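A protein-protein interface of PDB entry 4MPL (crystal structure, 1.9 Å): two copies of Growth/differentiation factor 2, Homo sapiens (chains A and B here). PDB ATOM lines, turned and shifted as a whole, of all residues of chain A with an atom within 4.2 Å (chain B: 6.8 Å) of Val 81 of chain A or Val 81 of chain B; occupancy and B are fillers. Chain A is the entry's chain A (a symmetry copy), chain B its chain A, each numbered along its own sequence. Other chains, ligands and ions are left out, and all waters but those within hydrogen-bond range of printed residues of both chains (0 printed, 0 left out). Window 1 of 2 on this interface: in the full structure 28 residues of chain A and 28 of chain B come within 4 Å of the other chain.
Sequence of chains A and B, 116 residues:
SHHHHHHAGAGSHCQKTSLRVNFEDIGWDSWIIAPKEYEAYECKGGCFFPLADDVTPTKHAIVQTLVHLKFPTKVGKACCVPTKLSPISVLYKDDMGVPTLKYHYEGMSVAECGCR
Cys 79 of chain B touches its own counterpart, Cys 79 of chain A.
Cys 79 of chain A touches Val 81 of chain B, and with the chains exchanged Val 81 of chain A touches Cys 79 of chain B.
Val 81 of chain A touches Arg 116 of chain B, and with the chains exchanged Arg 116 of chain A touches Val 81 of chain B.
Pro 82 of chain A touches Arg 116 of chain B, and with the chains exchanged Arg 116 of chain A touches Pro 82 of chain B.
Of the 8 pairs that touch across the chains among the printed residues, 8 have their exchanged pair printed and touching as well.
Of the printed residues of chain B, Cys 79 of chain A touches Cys 79 and Val 81.
Of the printed residues of chain B, Val 81 of chain A touches Cys 79 (3.8 Å), Val 81 (3.8 Å) and Arg 116 (3.97 Å).
Printed residues of chain B within 4 Å of Pro 82 of chain A: Arg 116.
Printed residues of chain B within 4 Å of Arg 116 of chain A: Val 81 (3.97 Å) and Pro 82 (3.3 Å).
Cys 43 of chain B touches none of the printed residues of chain A.
Printed residues of chain A within 4 Å of Pro 82 of chain B: Arg 116.
Of the printed residues of chain A, Arg 116 of chain B touches Val 81 (3.97 Å) and Pro 82 (3.3 Å).
The nearest printed residue of chain A that does not touch Val 81 of chain B is Cys 80 of chain A (6.0 Å).
The nearest printed residue of chain B that does not touch Arg 116 of chain A is Cys 80 of chain B (6.0 Å).
CB of Cys 79 of chain B touches CB of Cys 79 of chain A, at 3.8 Å.
Val 81 of chain B touches Cys 79 of chain A (CG1 to CB, 3.8 Å).
CB of Cys 79 of chain B touches CG1 of Val 81 of chain A, at 3.8 Å.
Val 81 of chain A touches Val 81 of chain B.
Arg 116 of chain B touches Val 81 of chain A (OXT to CG1, 3.97 Å).
Pro 82 of chain A touches Arg 116 of chain B.
CG1 of Val 81 of chain B touches OXT of Arg 116 of chain A, at 3.97 Å.
Arg 116 of chain A touches Pro 82 of chain B (O to CD, 3.3 Å).
Of the 17 printed residues of chain B, 4 touch a printed residue of chain A.
Hydrophobic or aromatic side chains of chain B within 4 Å of the printed part of chain A: Val 81 and Pro 82.
Among the printed residues, 8 pairs touch across the chains.
N of Val 81 of chain B lies within hydrogen-bond range of O of Gly 114 of chain B (2.9 Å).
N of Arg 116 of chain A lies within hydrogen-bond range of O of Cys 79 of chain A.
N of Val 81 of chain A sits at hydrogen-bond distance from O of Gly 114 of chain A, 2.9 Å away.
SG of Cys 80 of chain B is disulfide-bonded to SG of Cys 14 of chain B (2.0 Å).
The side-chain sulfur (SG) of Cys 47 of chain B forms a disulfide with the side-chain sulfur (SG) of Cys 115 of chain B, 2.0 Å away.
SG of Cys 113 of chain A forms a disulfide with SG of Cys 43 of chain A (2.0 Å).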
ATOM      1  N   CYS A  43     -18.467  -8.800 -20.724  1.00  0.00           N
ATOM      2  CA  CYS A  43     -18.038 -10.131 -20.315  1.00  0.00           C
ATOM      3  C   CYS A  43     -19.263 -11.003 -20.258  1.00  0.00           C
ATOM      4  O   CYS A  43     -20.207 -10.698 -19.532  1.00  0.00           O
ATOM      5  CB  CYS A  43     -17.377 -10.078 -18.942  1.00  0.00           C
ATOM      6  SG  CYS A  43     -15.888  -9.067 -18.918  1.00  0.00           S
ATOM      7  N   CYS A  79     -20.183 -14.391 -10.518  1.00  0.00           N
ATOM      8  CA  CYS A  79     -20.601 -13.638 -11.698  1.00  0.00           C
ATOM      9  C   CYS A  79     -19.430 -13.320 -12.620  1.00  0.00           C
ATOM     10  O   CYS A  79     -18.328 -12.999 -12.168  1.00  0.00           O
ATOM     11  CB  CYS A  79     -21.345 -12.360 -11.276  1.00  0.00           C
ATOM     12  SG  CYS A  79     -22.859 -12.677 -10.306  1.00  0.00           S
ATOM     13  N   CYS A  80     -19.673 -13.442 -13.919  1.00  0.00           N
ATOM     14  CA  CYS A  80     -18.681 -13.134 -14.939  1.00  0.00           C
ATOM     15  C   CYS A  80     -18.655 -11.612 -15.142  1.00  0.00           C
ATOM     16  O   CYS A  80     -19.636 -11.030 -15.621  1.00  0.00           O
ATOM     17  CB  CYS A  80     -19.100 -13.829 -16.239  1.00  0.00           C
ATOM     18  SG  CYS A  80     -18.023 -13.550 -17.624  1.00  0.00           S
ATOM     19  N   VAL A  81     -17.551 -10.964 -14.769  1.00  0.00           N
ATOM     20  CA  VAL A  81     -17.478  -9.498 -14.817  1.00  0.00           C
ATOM     21  C   VAL A  81     -16.147  -9.025 -15.373  1.00  0.00           C
ATOM     22  O   VAL A  81     -15.189  -9.783 -15.426  1.00  0.00           O
ATOM     23  CB  VAL A  81     -17.613  -8.870 -13.395  1.00  0.00           C
ATOM     24  CG1 VAL A  81     -19.011  -9.090 -12.825  1.00  0.00           C
ATOM     25  CG2 VAL A  81     -16.528  -9.446 -12.449  1.00  0.00           C
ATOM     26  N   PRO A  82     -16.073  -7.747 -15.767  1.00  0.00           N
ATOM     27  CA  PRO A  82     -14.758  -7.205 -16.130  1.00  0.00           C
ATOM     28  C   PRO A  82     -13.840  -7.151 -14.917  1.00  0.00           C
ATOM     29  O   PRO A  82     -14.234  -6.686 -13.847  1.00  0.00           O
ATOM     30  CB  PRO A  82     -15.083  -5.771 -16.581  1.00  0.00           C
ATOM     31  CG  PRO A  82     -16.533  -5.813 -16.994  1.00  0.00           C
ATOM     32  CD  PRO A  82     -17.170  -6.800 -16.035  1.00  0.00           C
ATOM     33  N   THR A  83     -12.612  -7.612 -15.077  1.00  0.00           N
ATOM     34  CA  THR A  83     -11.664  -7.593 -13.968  1.00  0.00           C
ATOM     35  C   THR A  83     -10.560  -6.569 -14.214  1.00  0.00           C
ATOM     36  O   THR A  83      -9.798  -6.225 -13.310  1.00  0.00           O
ATOM     37  CB  THR A  83     -11.063  -8.969 -13.769  1.00  0.00           C
ATOM     38  OG1 THR A  83     -10.616  -9.471 -15.041  1.00  0.00           O
ATOM     39  CG2 THR A  83     -12.132  -9.915 -13.204  1.00  0.00           C
ATOM     40  N   CYS A 113     -11.825 -10.285 -18.450  1.00  0.00           N
ATOM     41  CA  CYS A 113     -13.009 -10.783 -17.749  1.00  0.00           C
ATOM     42  C   CYS A 113     -12.613 -11.883 -16.778  1.00  0.00           C
ATOM     43  O   CYS A 113     -11.600 -12.545 -16.970  1.00  0.00           O
ATOM     44  CB  CYS A 113     -14.011 -11.376 -18.744  1.00  0.00           C
ATOM     45  SG  CYS A 113     -14.613 -10.210 -20.001  1.00  0.00           S
ATOM     46  N   GLY A 114     -13.419 -12.090 -15.748  1.00  0.00           N
ATOM     47  CA  GLY A 114     -13.189 -13.189 -14.817  1.00  0.00           C
ATOM     48  C   GLY A 114     -14.398 -13.441 -13.946  1.00  0.00           C
ATOM     49  O   GLY A 114     -15.338 -12.638 -13.930  1.00  0.00           O
ATOM     50  N   ARG A 116     -16.104 -13.604 -10.352  1.00  0.00           N
ATOM     51  CA  ARG A 116     -15.855 -12.960  -9.059  1.00  0.00           C
ATOM     52  C   ARG A 116     -17.009 -13.188  -8.073  1.00  0.00           C
ATOM     53  O   ARG A 116     -16.829 -13.156  -6.847  1.00  0.00           O
ATOM     54  CB  ARG A 116     -15.594 -11.456  -9.252  1.00  0.00           C
ATOM     55  CG  ARG A 116     -14.282 -11.116  -9.979  1.00  0.00           C
ATOM     56  CD  ARG A 116     -13.069 -11.586  -9.165  1.00  0.00           C
ATOM     57  NE  ARG A 116     -11.784 -11.184  -9.740  1.00  0.00           N
ATOM     58  CZ  ARG A 116     -11.074 -11.925 -10.596  1.00  0.00           C
ATOM     59  NH1 ARG A 116     -11.525 -13.105 -11.022  1.00  0.00           N
ATOM     60  NH2 ARG A 116      -9.916 -11.472 -11.051  1.00  0.00           N
ATOM     61  OXT ARG A 116     -18.159 -13.420  -8.472  1.00  0.00           O
ATOM     62  N   CYS B  14     -26.582  -3.082  -3.906  1.00  0.00           N
ATOM     63  CA  CYS B  14     -25.561  -4.131  -3.866  1.00  0.00           C
ATOM     64  C   CYS B  14     -24.797  -4.021  -2.549  1.00  0.00           C
ATOM     65  O   CYS B  14     -24.117  -3.026  -2.299  1.00  0.00           O
ATOM     66  CB  CYS B  14     -24.604  -3.967  -5.049  1.00  0.00           C
ATOM     67  SG  CYS B  14     -23.116  -4.988  -4.991  1.00  0.00           S
ATOM     68  N   CYS B  43     -22.054 -10.922  -1.716  1.00  0.00           N
ATOM     69  CA  CYS B  43     -22.579  -9.633  -2.148  1.00  0.00           C
ATOM     70  C   CYS B  43     -23.905  -9.885  -2.812  1.00  0.00           C
ATOM     71  O   CYS B  43     -23.980 -10.639  -3.780  1.00  0.00           O
ATOM     72  CB  CYS B  43     -21.624  -8.974  -3.137  1.00  0.00           C
ATOM     73  SG  CYS B  43     -20.010  -8.618  -2.422  1.00  0.00           S
ATOM     74  N   LYS B  44     -24.974  -9.300  -2.286  1.00  0.00           N
ATOM     75  CA  LYS B  44     -26.242  -9.434  -2.994  1.00  0.00           C
ATOM     76  C   LYS B  44     -26.990  -8.113  -3.145  1.00  0.00           C
ATOM     77  O   LYS B  44     -26.699  -7.113  -2.470  1.00  0.00           O
ATOM     78  CB  LYS B  44     -27.122 -10.533  -2.390  1.00  0.00           C
ATOM     79  CG  LYS B  44     -27.934 -10.134  -1.179  1.00  0.00           C
ATOM     80  CD  LYS B  44     -28.774 -11.324  -0.689  1.00  0.00           C
ATOM     81  CE  LYS B  44     -29.501 -10.992   0.609  1.00  0.00           C
ATOM     82  NZ  LYS B  44     -30.321 -12.134   1.113  1.00  0.00           N
ATOM     83  N   CYS B  47     -27.839  -3.896  -9.316  1.00  0.00           N
ATOM     84  CA  CYS B  47     -27.143  -2.753  -9.875  1.00  0.00           C
ATOM     85  C   CYS B  47     -28.117  -2.200 -10.899  1.00  0.00           C
ATOM     86  O   CYS B  47     -28.166  -2.654 -12.050  1.00  0.00           O
ATOM     87  CB  CYS B  47     -25.860  -3.191 -10.566  1.00  0.00           C
ATOM     88  SG  CYS B  47     -24.793  -4.140  -9.495  1.00  0.00           S
ATOM     89  N   ALA B  78     -25.176  -5.053 -15.104  1.00  0.00           N
ATOM     90  CA  ALA B  78     -23.950  -5.042 -14.302  1.00  0.00           C
ATOM     91  C   ALA B  78     -24.201  -5.998 -13.146  1.00  0.00           C
ATOM     92  O   ALA B  78     -25.351  -6.212 -12.749  1.00  0.00           O
ATOM     93  CB  ALA B  78     -23.679  -3.662 -13.762  1.00  0.00           C
ATOM     94  N   CYS B  79     -23.139  -6.565 -12.588  1.00  0.00           N
ATOM     95  CA  CYS B  79     -23.307  -7.577 -11.548  1.00  0.00           C
ATOM     96  C   CYS B  79     -22.732  -7.126 -10.211  1.00  0.00           C
ATOM     97  O   CYS B  79     -21.674  -6.495 -10.149  1.00  0.00           O
ATOM     98  CB  CYS B  79     -22.692  -8.911 -12.001  1.00  0.00           C
ATOM     99  SG  CYS B  79     -23.453  -9.597 -13.512  1.00  0.00           S
ATOM    100  N   CYS B  80     -23.459  -7.430  -9.142  1.00  0.00           N
ATOM    101  CA  CYS B  80     -23.035  -7.114  -7.786  1.00  0.00           C
ATOM    102  C   CYS B  80     -22.024  -8.179  -7.336  1.00  0.00           C
ATOM    103  O   CYS B  80     -22.384  -9.352  -7.176  1.00  0.00           O
ATOM    104  CB  CYS B  80     -24.270  -7.148  -6.879  1.00  0.00           C
ATOM    105  SG  CYS B  80     -23.955  -6.814  -5.163  1.00  0.00           S
ATOM    106  N   VAL B  81     -20.764  -7.786  -7.146  1.00  0.00           N
ATOM    107  CA  VAL B  81     -19.706  -8.754  -6.829  1.00  0.00           C
ATOM    108  C   VAL B  81     -18.787  -8.236  -5.738  1.00  0.00           C
ATOM    109  O   VAL B  81     -18.767  -7.046  -5.453  1.00  0.00           O
ATOM    110  CB  VAL B  81     -18.804  -9.044  -8.069  1.00  0.00           C
ATOM    111  CG1 VAL B  81     -19.579  -9.781  -9.156  1.00  0.00           C
ATOM    112  CG2 VAL B  81     -18.199  -7.723  -8.613  1.00  0.00           C
ATOM    113  N   PRO B  82     -17.992  -9.131  -5.137  1.00  0.00           N
ATOM    114  CA  PRO B  82     -16.960  -8.639  -4.216  1.00  0.00           C
ATOM    115  C   PRO B  82     -15.910  -7.826  -4.962  1.00  0.00           C
ATOM    116  O   PRO B  82     -15.412  -8.245  -6.006  1.00  0.00           O
ATOM    117  CB  PRO B  82     -16.316  -9.931  -3.690  1.00  0.00           C
ATOM    118  CG  PRO B  82     -17.371 -10.994  -3.872  1.00  0.00           C
ATOM    119  CD  PRO B  82     -18.084 -10.602  -5.152  1.00  0.00           C
ATOM    120  N   THR B  83     -15.561  -6.669  -4.426  1.00  0.00           N
ATOM    121  CA  THR B  83     -14.558  -5.829  -5.071  1.00  0.00           C
ATOM    122  C   THR B  83     -13.269  -5.798  -4.256  1.00  0.00           C
ATOM    123  O   THR B  83     -12.226  -5.347  -4.730  1.00  0.00           O
ATOM    124  CB  THR B  83     -15.092  -4.423  -5.254  1.00  0.00           C
ATOM    125  OG1 THR B  83     -15.661  -3.975  -4.011  1.00  0.00           O
ATOM    126  CG2 THR B  83     -16.183  -4.429  -6.333  1.00  0.00           C
ATOM    127  N   LYS B  84     -13.354  -6.278  -3.022  1.00  0.00           N
ATOM    128  CA  LYS B  84     -12.182  -6.418  -2.165  1.00  0.00           C
ATOM    129  C   LYS B  84     -12.386  -7.648  -1.282  1.00  0.00           C
ATOM    130  O   LYS B  84     -13.495  -7.873  -0.786  1.00  0.00           O
ATOM    131  CB  LYS B  84     -11.991  -5.163  -1.300  1.00  0.00           C
ATOM    132  CG  LYS B  84     -10.815  -5.261  -0.330  1.00  0.00           C
ATOM    133  CD  LYS B  84     -10.284  -3.895   0.089  1.00  0.00           C
ATOM    134  CE  LYS B  84      -9.284  -4.020   1.237  1.00  0.00           C
ATOM    135  NZ  LYS B  84      -9.963  -4.178   2.559  1.00  0.00           N
ATOM    136  N   VAL B 110     -15.445 -11.664   1.891  1.00  0.00           N
ATOM    137  CA  VAL B 110     -15.733 -10.385   1.245  1.00  0.00           C
ATOM    138  C   VAL B 110     -15.406  -9.235   2.186  1.00  0.00           C
ATOM    139  O   VAL B 110     -15.838  -9.225   3.343  1.00  0.00           O
ATOM    140  CB  VAL B 110     -17.195 -10.260   0.813  1.00  0.00           C
ATOM    141  CG1 VAL B 110     -17.424  -8.904   0.147  1.00  0.00           C
ATOM    142  CG2 VAL B 110     -17.570 -11.388  -0.143  1.00  0.00           C
ATOM    143  N   GLU B 112     -15.465  -5.828   0.587  1.00  0.00           N
ATOM    144  CA  GLU B 112     -16.329  -4.817  -0.028  1.00  0.00           C
ATOM    145  C   GLU B 112     -17.061  -5.363  -1.250  1.00  0.00           C
ATOM    146  O   GLU B 112     -16.543  -6.230  -1.945  1.00  0.00           O
ATOM    147  CB  GLU B 112     -15.503  -3.596  -0.440  1.00  0.00           C
ATOM    148  CG  GLU B 112     -14.914  -2.827   0.736  1.00  0.00           C
ATOM    149  CD  GLU B 112     -14.339  -1.490   0.322  1.00  0.00           C
ATOM    150  OE1 GLU B 112     -13.940  -1.358  -0.855  1.00  0.00           O
ATOM    151  OE2 GLU B 112     -14.291  -0.571   1.171  1.00  0.00           O
ATOM    152  N   CYS B 113     -18.256  -4.837  -1.507  1.00  0.00           N
ATOM    153  CA  CYS B 113     -19.049  -5.210  -2.679  1.00  0.00           C
ATOM    154  C   CYS B 113     -19.218  -4.010  -3.595  1.00  0.00           C
ATOM    155  O   CYS B 113     -19.151  -2.872  -3.146  1.00  0.00           O
ATOM    156  CB  CYS B 113     -20.446  -5.674  -2.253  1.00  0.00           C
ATOM    157  SG  CYS B 113     -20.463  -7.112  -1.144  1.00  0.00           S
ATOM    158  N   GLY B 114     -19.455  -4.263  -4.873  1.00  0.00           N
ATOM    159  CA  GLY B 114     -19.737  -3.186  -5.816  1.00  0.00           C
ATOM    160  C   GLY B 114     -20.308  -3.718  -7.111  1.00  0.00           C
ATOM    161  O   GLY B 114     -20.299  -4.932  -7.349  1.00  0.00           O
ATOM    162  N   CYS B 115     -20.812  -2.817  -7.954  1.00  0.00           N
ATOM    163  CA  CYS B 115     -21.355  -3.218  -9.239  1.00  0.00           C
ATOM    164  C   CYS B 115     -20.238  -3.146 -10.275  1.00  0.00           C
ATOM    165  O   CYS B 115     -19.514  -2.154 -10.350  1.00  0.00           O
ATOM    166  CB  CYS B 115     -22.530  -2.318  -9.626  1.00  0.00           C
ATOM    167  SG  CYS B 115     -23.975  -2.584  -8.533  1.00  0.00           S
ATOM    168  N   ARG B 116     -20.077  -4.206 -11.056  1.00  0.00           N
ATOM    169  CA  ARG B 116     -18.982  -4.258 -12.030  1.00  0.00           C
ATOM    170  C   ARG B 116     -19.460  -4.748 -13.404  1.00  0.00           C
ATOM    171  O   ARG B 116     -18.863  -4.439 -14.445  1.00  0.00           O
ATOM    172  CB  ARG B 116     -17.840  -5.143 -11.503  1.00  0.00           C
ATOM    173  CG  ARG B 116     -17.091  -4.575 -10.285  1.00  0.00           C
ATOM    174  CD  ARG B 116     -16.385  -3.261 -10.643  1.00  0.00           C
ATOM    175  NE  ARG B 116     -15.551  -2.729  -9.564  1.00  0.00           N
ATOM    176  CZ  ARG B 116     -15.974  -1.861  -8.639  1.00  0.00           C
ATOM    177  NH1 ARG B 116     -17.237  -1.436  -8.622  1.00  0.00           N
ATOM    178  NH2 ARG B 116     -15.134  -1.433  -7.709  1.00  0.00           N
ATOM    179  OXT ARG B 116     -20.464  -5.466 -13.517  1.00  0.00           O
